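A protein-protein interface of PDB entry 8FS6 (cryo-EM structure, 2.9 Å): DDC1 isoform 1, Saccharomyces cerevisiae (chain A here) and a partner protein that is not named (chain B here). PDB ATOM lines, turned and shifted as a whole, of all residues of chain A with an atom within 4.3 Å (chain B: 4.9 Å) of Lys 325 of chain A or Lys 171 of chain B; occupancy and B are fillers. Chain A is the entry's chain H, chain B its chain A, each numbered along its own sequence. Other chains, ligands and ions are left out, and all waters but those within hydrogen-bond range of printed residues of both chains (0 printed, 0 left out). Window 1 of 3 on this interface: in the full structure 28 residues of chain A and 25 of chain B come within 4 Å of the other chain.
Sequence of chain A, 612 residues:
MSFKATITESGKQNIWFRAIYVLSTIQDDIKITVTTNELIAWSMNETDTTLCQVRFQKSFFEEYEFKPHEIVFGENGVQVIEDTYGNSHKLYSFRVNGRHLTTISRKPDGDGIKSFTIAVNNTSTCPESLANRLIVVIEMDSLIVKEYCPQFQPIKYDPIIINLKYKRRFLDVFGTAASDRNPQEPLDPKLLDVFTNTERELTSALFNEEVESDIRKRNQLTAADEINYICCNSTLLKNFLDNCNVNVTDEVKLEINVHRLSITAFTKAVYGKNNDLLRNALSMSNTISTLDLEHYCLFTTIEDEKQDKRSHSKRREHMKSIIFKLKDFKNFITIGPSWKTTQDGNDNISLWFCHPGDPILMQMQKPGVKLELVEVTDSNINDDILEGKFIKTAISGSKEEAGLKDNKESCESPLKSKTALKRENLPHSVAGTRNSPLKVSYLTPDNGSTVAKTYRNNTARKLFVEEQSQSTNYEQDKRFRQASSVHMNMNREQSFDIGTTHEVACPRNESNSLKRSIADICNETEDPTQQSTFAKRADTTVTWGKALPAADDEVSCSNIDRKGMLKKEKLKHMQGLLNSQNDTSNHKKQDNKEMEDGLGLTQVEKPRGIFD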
ATOM      1  N   ASP A 250     -29.237  11.850   0.075  1.00  0.00           N
ATOM      2  CA  ASP A 250     -28.857  13.252  -0.038  1.00  0.00           C
ATOM      3  C   ASP A 250     -27.559  13.443  -0.817  1.00  0.00           C
ATOM      4  O   ASP A 250     -26.945  14.513  -0.728  1.00  0.00           O
ATOM      5  CB  ASP A 250     -28.730  13.893   1.348  1.00  0.00           C
ATOM      6  CG  ASP A 250     -29.984  14.640   1.760  1.00  0.00           C
ATOM      7  OD1 ASP A 250     -30.818  14.934   0.879  1.00  0.00           O
ATOM      8  OD2 ASP A 250     -30.139  14.928   2.965  1.00  0.00           O
ATOM      9  N   VAL A 252     -25.790  13.228  -4.695  1.00  0.00           N
ATOM     10  CA  VAL A 252     -26.047  13.185  -6.130  1.00  0.00           C
ATOM     11  C   VAL A 252     -24.712  13.055  -6.847  1.00  0.00           C
ATOM     12  O   VAL A 252     -23.819  13.893  -6.668  1.00  0.00           O
ATOM     13  CB  VAL A 252     -26.804  14.433  -6.609  1.00  0.00           C
ATOM     14  CG1 VAL A 252     -26.835  14.485  -8.130  1.00  0.00           C
ATOM     15  CG2 VAL A 252     -28.206  14.444  -6.045  1.00  0.00           C
ATOM     16  N   ARG A 279     -26.219   2.909   8.955  1.00  0.00           N
ATOM     17  CA  ARG A 279     -26.932   3.581   7.877  1.00  0.00           C
ATOM     18  C   ARG A 279     -26.887   2.701   6.638  1.00  0.00           C
ATOM     19  O   ARG A 279     -25.814   2.232   6.245  1.00  0.00           O
ATOM     20  CB  ARG A 279     -26.321   4.956   7.579  1.00  0.00           C
ATOM     21  CG  ARG A 279     -27.001   5.712   6.450  1.00  0.00           C
ATOM     22  CD  ARG A 279     -26.365   7.078   6.242  1.00  0.00           C
ATOM     23  NE  ARG A 279     -27.041   7.845   5.202  1.00  0.00           N
ATOM     24  CZ  ARG A 279     -28.063   8.662   5.417  1.00  0.00           C
ATOM     25  NH1 ARG A 279     -28.557   8.846   6.630  1.00  0.00           N
ATOM     26  NH2 ARG A 279     -28.602   9.311   4.388  1.00  0.00           N
ATOM     27  N   PHE A 324     -22.528  16.215  -5.055  1.00  0.00           N
ATOM     28  CA  PHE A 324     -23.068  17.298  -4.240  1.00  0.00           C
ATOM     29  C   PHE A 324     -24.354  16.807  -3.581  1.00  0.00           C
ATOM     30  O   PHE A 324     -24.672  15.615  -3.614  1.00  0.00           O
ATOM     31  CB  PHE A 324     -23.282  18.566  -5.080  1.00  0.00           C
ATOM     32  CG  PHE A 324     -23.956  18.322  -6.402  1.00  0.00           C
ATOM     33  CD1 PHE A 324     -23.211  18.041  -7.537  1.00  0.00           C
ATOM     34  CD2 PHE A 324     -25.334  18.388  -6.512  1.00  0.00           C
ATOM     35  CE1 PHE A 324     -23.832  17.820  -8.753  1.00  0.00           C
ATOM     36  CE2 PHE A 324     -25.960  18.169  -7.724  1.00  0.00           C
ATOM     37  CZ  PHE A 324     -25.207  17.885  -8.846  1.00  0.00           C
ATOM     38  N   LYS A 325     -25.097  17.733  -2.979  1.00  0.00           N
ATOM     39  CA  LYS A 325     -26.300  17.388  -2.236  1.00  0.00           C
ATOM     40  C   LYS A 325     -27.482  17.194  -3.187  1.00  0.00           C
ATOM     41  O   LYS A 325     -27.353  17.269  -4.411  1.00  0.00           O
ATOM     42  CB  LYS A 325     -26.602  18.459  -1.190  1.00  0.00           C
ATOM     43  CG  LYS A 325     -25.538  18.583  -0.110  1.00  0.00           C
ATOM     44  CD  LYS A 325     -26.001  17.968   1.200  1.00  0.00           C
ATOM     45  CE  LYS A 325     -27.222  18.688   1.750  1.00  0.00           C
ATOM     46  NZ  LYS A 325     -27.921  17.883   2.788  1.00  0.00           N
ATOM     47  N   LEU A 326     -28.656  16.938  -2.613  1.00  0.00           N
ATOM     48  CA  LEU A 326     -29.854  16.635  -3.388  1.00  0.00           C
ATOM     49  C   LEU A 326     -31.001  17.601  -3.145  1.00  0.00           C
ATOM     50  O   LEU A 326     -31.678  17.994  -4.099  1.00  0.00           O
ATOM     51  CB  LEU A 326     -30.324  15.201  -3.086  1.00  0.00           C
ATOM     52  CG  LEU A 326     -31.690  14.781  -3.638  1.00  0.00           C
ATOM     53  CD1 LEU A 326     -31.681  14.781  -5.153  1.00  0.00           C
ATOM     54  CD2 LEU A 326     -32.092  13.414  -3.115  1.00  0.00           C
ATOM     55  N   LYS A 327     -31.242  17.995  -1.890  1.00  0.00           N
ATOM     56  CA  LYS A 327     -32.412  18.815  -1.577  1.00  0.00           C
ATOM     57  C   LYS A 327     -32.333  20.184  -2.244  1.00  0.00           C
ATOM     58  O   LYS A 327     -33.324  20.665  -2.811  1.00  0.00           O
ATOM     59  CB  LYS A 327     -32.556  18.957  -0.060  1.00  0.00           C
ATOM     60  CG  LYS A 327     -33.087  20.304   0.408  1.00  0.00           C
ATOM     61  CD  LYS A 327     -32.971  20.452   1.917  1.00  0.00           C
ATOM     62  CE  LYS A 327     -33.977  19.569   2.636  1.00  0.00           C
ATOM     63  NZ  LYS A 327     -35.343  20.161   2.620  1.00  0.00           N
ATOM     64  N   ASP A 328     -31.161  20.826  -2.191  1.00  0.00           N
ATOM     65  CA  ASP A 328     -31.004  22.132  -2.825  1.00  0.00           C
ATOM     66  C   ASP A 328     -31.183  22.035  -4.333  1.00  0.00           C
ATOM     67  O   ASP A 328     -31.867  22.869  -4.942  1.00  0.00           O
ATOM     68  CB  ASP A 328     -29.634  22.719  -2.487  1.00  0.00           C
ATOM     69  CG  ASP A 328     -29.168  22.344  -1.095  1.00  0.00           C
ATOM     70  OD1 ASP A 328     -29.834  22.741  -0.116  1.00  0.00           O
ATOM     71  OD2 ASP A 328     -28.134  21.651  -0.980  1.00  0.00           O
ATOM     72  N   PHE A 329     -30.582  21.013  -4.951  1.00  0.00           N
ATOM     73  CA  PHE A 329     -30.742  20.812  -6.387  1.00  0.00           C
ATOM     74  C   PHE A 329     -32.195  20.534  -6.742  1.00  0.00           C
ATOM     75  O   PHE A 329     -32.710  21.068  -7.730  1.00  0.00           O
ATOM     76  CB  PHE A 329     -29.847  19.667  -6.862  1.00  0.00           C
ATOM     77  CG  PHE A 329     -29.781  19.531  -8.357  1.00  0.00           C
ATOM     78  CD1 PHE A 329     -29.770  20.653  -9.171  1.00  0.00           C
ATOM     79  CD2 PHE A 329     -29.730  18.280  -8.950  1.00  0.00           C
ATOM     80  CE1 PHE A 329     -29.708  20.529 -10.547  1.00  0.00           C
ATOM     81  CE2 PHE A 329     -29.668  18.150 -10.325  1.00  0.00           C
ATOM     82  CZ  PHE A 329     -29.658  19.276 -11.124  1.00  0.00           C
ATOM     83  N   GLU A 375     -23.464  25.340  -5.237  1.00  0.00           N
ATOM     84  CA  GLU A 375     -23.384  24.168  -4.378  1.00  0.00           C
ATOM     85  C   GLU A 375     -21.945  23.686  -4.306  1.00  0.00           C
ATOM     86  O   GLU A 375     -21.285  23.540  -5.339  1.00  0.00           O
ATOM     87  CB  GLU A 375     -24.294  23.042  -4.885  1.00  0.00           C
ATOM     88  CG  GLU A 375     -25.256  22.510  -3.835  1.00  0.00           C
ATOM     89  CD  GLU A 375     -26.271  21.543  -4.410  1.00  0.00           C
ATOM     90  OE1 GLU A 375     -26.618  20.562  -3.720  1.00  0.00           O
ATOM     91  OE2 GLU A 375     -26.724  21.764  -5.554  1.00  0.00           O
ATOM     92  N   GLU B 164     -34.473  16.844  12.108  1.00  0.00           N
ATOM     93  CA  GLU B 164     -33.523  16.654  11.023  1.00  0.00           C
ATOM     94  C   GLU B 164     -32.617  17.857  10.802  1.00  0.00           C
ATOM     95  O   GLU B 164     -31.808  17.839   9.868  1.00  0.00           O
ATOM     96  CB  GLU B 164     -34.271  16.327   9.724  1.00  0.00           C
ATOM     97  CG  GLU B 164     -33.554  15.339   8.817  1.00  0.00           C
ATOM     98  CD  GLU B 164     -34.290  15.112   7.510  1.00  0.00           C
ATOM     99  OE1 GLU B 164     -35.268  15.840   7.245  1.00  0.00           O
ATOM    100  OE2 GLU B 164     -33.890  14.204   6.751  1.00  0.00           O
ATOM    101  N   SER B 167     -29.140  16.716  11.452  1.00  0.00           N
ATOM    102  CA  SER B 167     -28.756  15.787  10.395  1.00  0.00           C
ATOM    103  C   SER B 167     -28.360  16.535   9.127  1.00  0.00           C
ATOM    104  O   SER B 167     -27.345  16.221   8.496  1.00  0.00           O
ATOM    105  CB  SER B 167     -29.900  14.812  10.114  1.00  0.00           C
ATOM    106  OG  SER B 167     -29.478  13.765   9.258  1.00  0.00           O
ATOM    107  N   GLU B 168     -29.152  17.542   8.747  1.00  0.00           N
ATOM    108  CA  GLU B 168     -28.812  18.354   7.582  1.00  0.00           C
ATOM    109  C   GLU B 168     -27.531  19.146   7.816  1.00  0.00           C
ATOM    110  O   GLU B 168     -26.720  19.310   6.896  1.00  0.00           O
ATOM    111  CB  GLU B 168     -29.969  19.291   7.236  1.00  0.00           C
ATOM    112  CG  GLU B 168     -31.207  18.578   6.721  1.00  0.00           C
ATOM    113  CD  GLU B 168     -31.008  17.992   5.336  1.00  0.00           C
ATOM    114  OE1 GLU B 168     -31.115  16.756   5.192  1.00  0.00           O
ATOM    115  OE2 GLU B 168     -30.744  18.766   4.393  1.00  0.00           O
ATOM    116  N   PHE B 169     -27.333  19.644   9.040  1.00  0.00           N
ATOM    117  CA  PHE B 169     -26.101  20.359   9.360  1.00  0.00           C
ATOM    118  C   PHE B 169     -24.883  19.454   9.218  1.00  0.00           C
ATOM    119  O   PHE B 169     -23.853  19.869   8.673  1.00  0.00           O
ATOM    120  CB  PHE B 169     -26.184  20.931  10.776  1.00  0.00           C
ATOM    121  CG  PHE B 169     -24.915  21.583  11.244  1.00  0.00           C
ATOM    122  CD1 PHE B 169     -24.572  22.850  10.807  1.00  0.00           C
ATOM    123  CD2 PHE B 169     -24.068  20.930  12.124  1.00  0.00           C
ATOM    124  CE1 PHE B 169     -23.405  23.455  11.234  1.00  0.00           C
ATOM    125  CE2 PHE B 169     -22.901  21.528  12.555  1.00  0.00           C
ATOM    126  CZ  PHE B 169     -22.569  22.792  12.110  1.00  0.00           C
ATOM    127  N   LEU B 170     -24.982  18.213   9.700  1.00  0.00           N
ATOM    128  CA  LEU B 170     -23.876  17.270   9.563  1.00  0.00           C
ATOM    129  C   LEU B 170     -23.642  16.895   8.105  1.00  0.00           C
ATOM    130  O   LEU B 170     -22.492  16.764   7.671  1.00  0.00           O
ATOM    131  CB  LEU B 170     -24.141  16.017  10.398  1.00  0.00           C
ATOM    132  CG  LEU B 170     -23.779  16.076  11.881  1.00  0.00           C
ATOM    133  CD1 LEU B 170     -23.893  14.694  12.501  1.00  0.00           C
ATOM    134  CD2 LEU B 170     -22.382  16.644  12.077  1.00  0.00           C
ATOM    135  N   LYS B 171     -24.719  16.701   7.339  1.00  0.00           N
ATOM    136  CA  LYS B 171     -24.572  16.349   5.930  1.00  0.00           C
ATOM    137  C   LYS B 171     -23.911  17.474   5.144  1.00  0.00           C
ATOM    138  O   LYS B 171     -23.078  17.222   4.266  1.00  0.00           O
ATOM    139  CB  LYS B 171     -25.934  16.000   5.330  1.00  0.00           C
ATOM    140  CG  LYS B 171     -26.501  14.676   5.816  1.00  0.00           C
ATOM    141  CD  LYS B 171     -27.907  14.449   5.290  1.00  0.00           C
ATOM    142  CE  LYS B 171     -28.432  13.079   5.687  1.00  0.00           C
ATOM    143  NZ  LYS B 171     -29.814  12.847   5.182  1.00  0.00           N
ATOM    144  N   GLY B 172     -24.268  18.725   5.444  1.00  0.00           N
ATOM    145  CA  GLY B 172     -23.631  19.851   4.786  1.00  0.00           C
ATOM    146  C   GLY B 172     -22.261  20.201   5.323  1.00  0.00           C
ATOM    147  O   GLY B 172     -21.498  20.892   4.640  1.00  0.00           O
ATOM    148  N   ALA B 173     -21.927  19.739   6.528  1.00  0.00           N
ATOM    149  CA  ALA B 173     -20.638  20.034   7.136  1.00  0.00           C
ATOM    150  C   ALA B 173     -19.565  19.007   6.800  1.00  0.00           C
ATOM    151  O   ALA B 173     -18.393  19.237   7.115  1.00  0.00           O
ATOM    152  CB  ALA B 173     -20.783  20.135   8.658  1.00  0.00           C
ATOM    153  N   ARG B 174     -19.930  17.890   6.170  1.00  0.00           N
ATOM    154  CA  ARG B 174     -18.942  16.898   5.766  1.00  0.00           C
ATOM    155  C   ARG B 174     -18.192  17.299   4.505  1.00  0.00           C
ATOM    156  O   ARG B 174     -17.162  16.690   4.195  1.00  0.00           O
ATOM    157  CB  ARG B 174     -19.612  15.537   5.555  1.00  0.00           C
ATOM    158  CG  ARG B 174     -20.227  15.352   4.178  1.00  0.00           C
ATOM    159  CD  ARG B 174     -20.312  13.880   3.806  1.00  0.00           C
ATOM    160  NE  ARG B 174     -20.500  13.686   2.373  1.00  0.00           N
ATOM    161  CZ  ARG B 174     -19.523  13.713   1.477  1.00  0.00           C
ATOM    162  NH1 ARG B 174     -18.265  13.924   1.832  1.00  0.00           N
ATOM    163  NH2 ARG B 174     -19.813  13.526   0.194  1.00  0.00           N
ATOM    164  N   TYR B 175     -18.677  18.303   3.779  1.00  0.00           N
ATOM    165  CA  TYR B 175     -18.008  18.808   2.589  1.00  0.00           C
ATOM    166  C   TYR B 175     -16.971  19.874   2.908  1.00  0.00           C
ATOM    167  O   TYR B 175     -16.317  20.378   1.989  1.00  0.00           O
ATOM    168  CB  TYR B 175     -19.038  19.374   1.606  1.00  0.00           C
ATOM    169  CG  TYR B 175     -19.945  18.332   0.991  1.00  0.00           C
ATOM    170  CD1 TYR B 175     -21.091  17.904   1.648  1.00  0.00           C
ATOM    171  CD2 TYR B 175     -19.657  17.780  -0.250  1.00  0.00           C
ATOM    172  CE1 TYR B 175     -21.922  16.952   1.089  1.00  0.00           C
ATOM    173  CE2 TYR B 175     -20.483  16.828  -0.818  1.00  0.00           C
ATOM    174  CZ  TYR B 175     -21.613  16.418  -0.144  1.00  0.00           C
ATOM    175  OH  TYR B 175     -22.438  15.471  -0.706  1.00  0.00           O
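NZ of Lys 171 of chain B lies within salt-bridge range of OD2 of Asp 250 of chain A. OE1 of Glu 168 of chain B sits close to OD2 of Asp 250 of chain A. The side-chain amino group (NZ) of Lys 325 of chain A lies within salt-bridge range of the side-chain carboxylate (OE2) of Glu 168 of chain B, at 3.4 Å.
N of Val 252 of chain A lies within hydrogen-bond range of O of Phe 324 of chain A (2.8 Å). The side-chain hydroxyl (OH) of Tyr 175 of chain B sits at hydrogen-bond distance from the guanidinium group (NH2) of Arg 174 of chain B. The side-chain carboxylate (OE1) of Glu 375 of chain A lies close to the backbone NH (N) of Lys 325 of chain A (3.3 Å). OD2 of Asp 250 of chain A lies within salt-bridge range of NZ of Lys 325 of chain A.
Among the printed residues, merely in contact across the chains: Phe 324 of chain A with Tyr 175 of chain B (3.7 Å), Lys 327 of chain A with Glu 168 of chain B (3.7 Å), Lys 325 of chain A with Lys 171 of chain B (3.7 Å) and Arg 279 of chain A with Lys 171 of chain B (3.8 Å).
Of chain B, only Glu 168 and Lys 171 come within 4 Å of Lys 325 of chain A. Lys 171 of chain B touches three residues of chain A. Of the printed residues of chain A, Tyr 175 of chain B touches Phe 324. Printed residues of chain B within 4 Å of Phe 324 of chain A: Tyr 175. Ser 167 of chain B touches none of the printed residues of chain A. Val 252 of chain A touches none of the printed residues of chain B. The nearest residue of chain B that does not touch Lys 325 of chain A is Tyr 175 of chain B (4.1 Å).
Of the 10 printed residues of chain A, 5 touch a printed residue of chain B. Of the 10 printed residues of chain B, 3 touch a printed residue of chain A. Hydrophobic or aromatic side chains of chain B that line the printed part of chain A: Tyr 175. Among the printed residues, 7 pairs touch across the chains.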
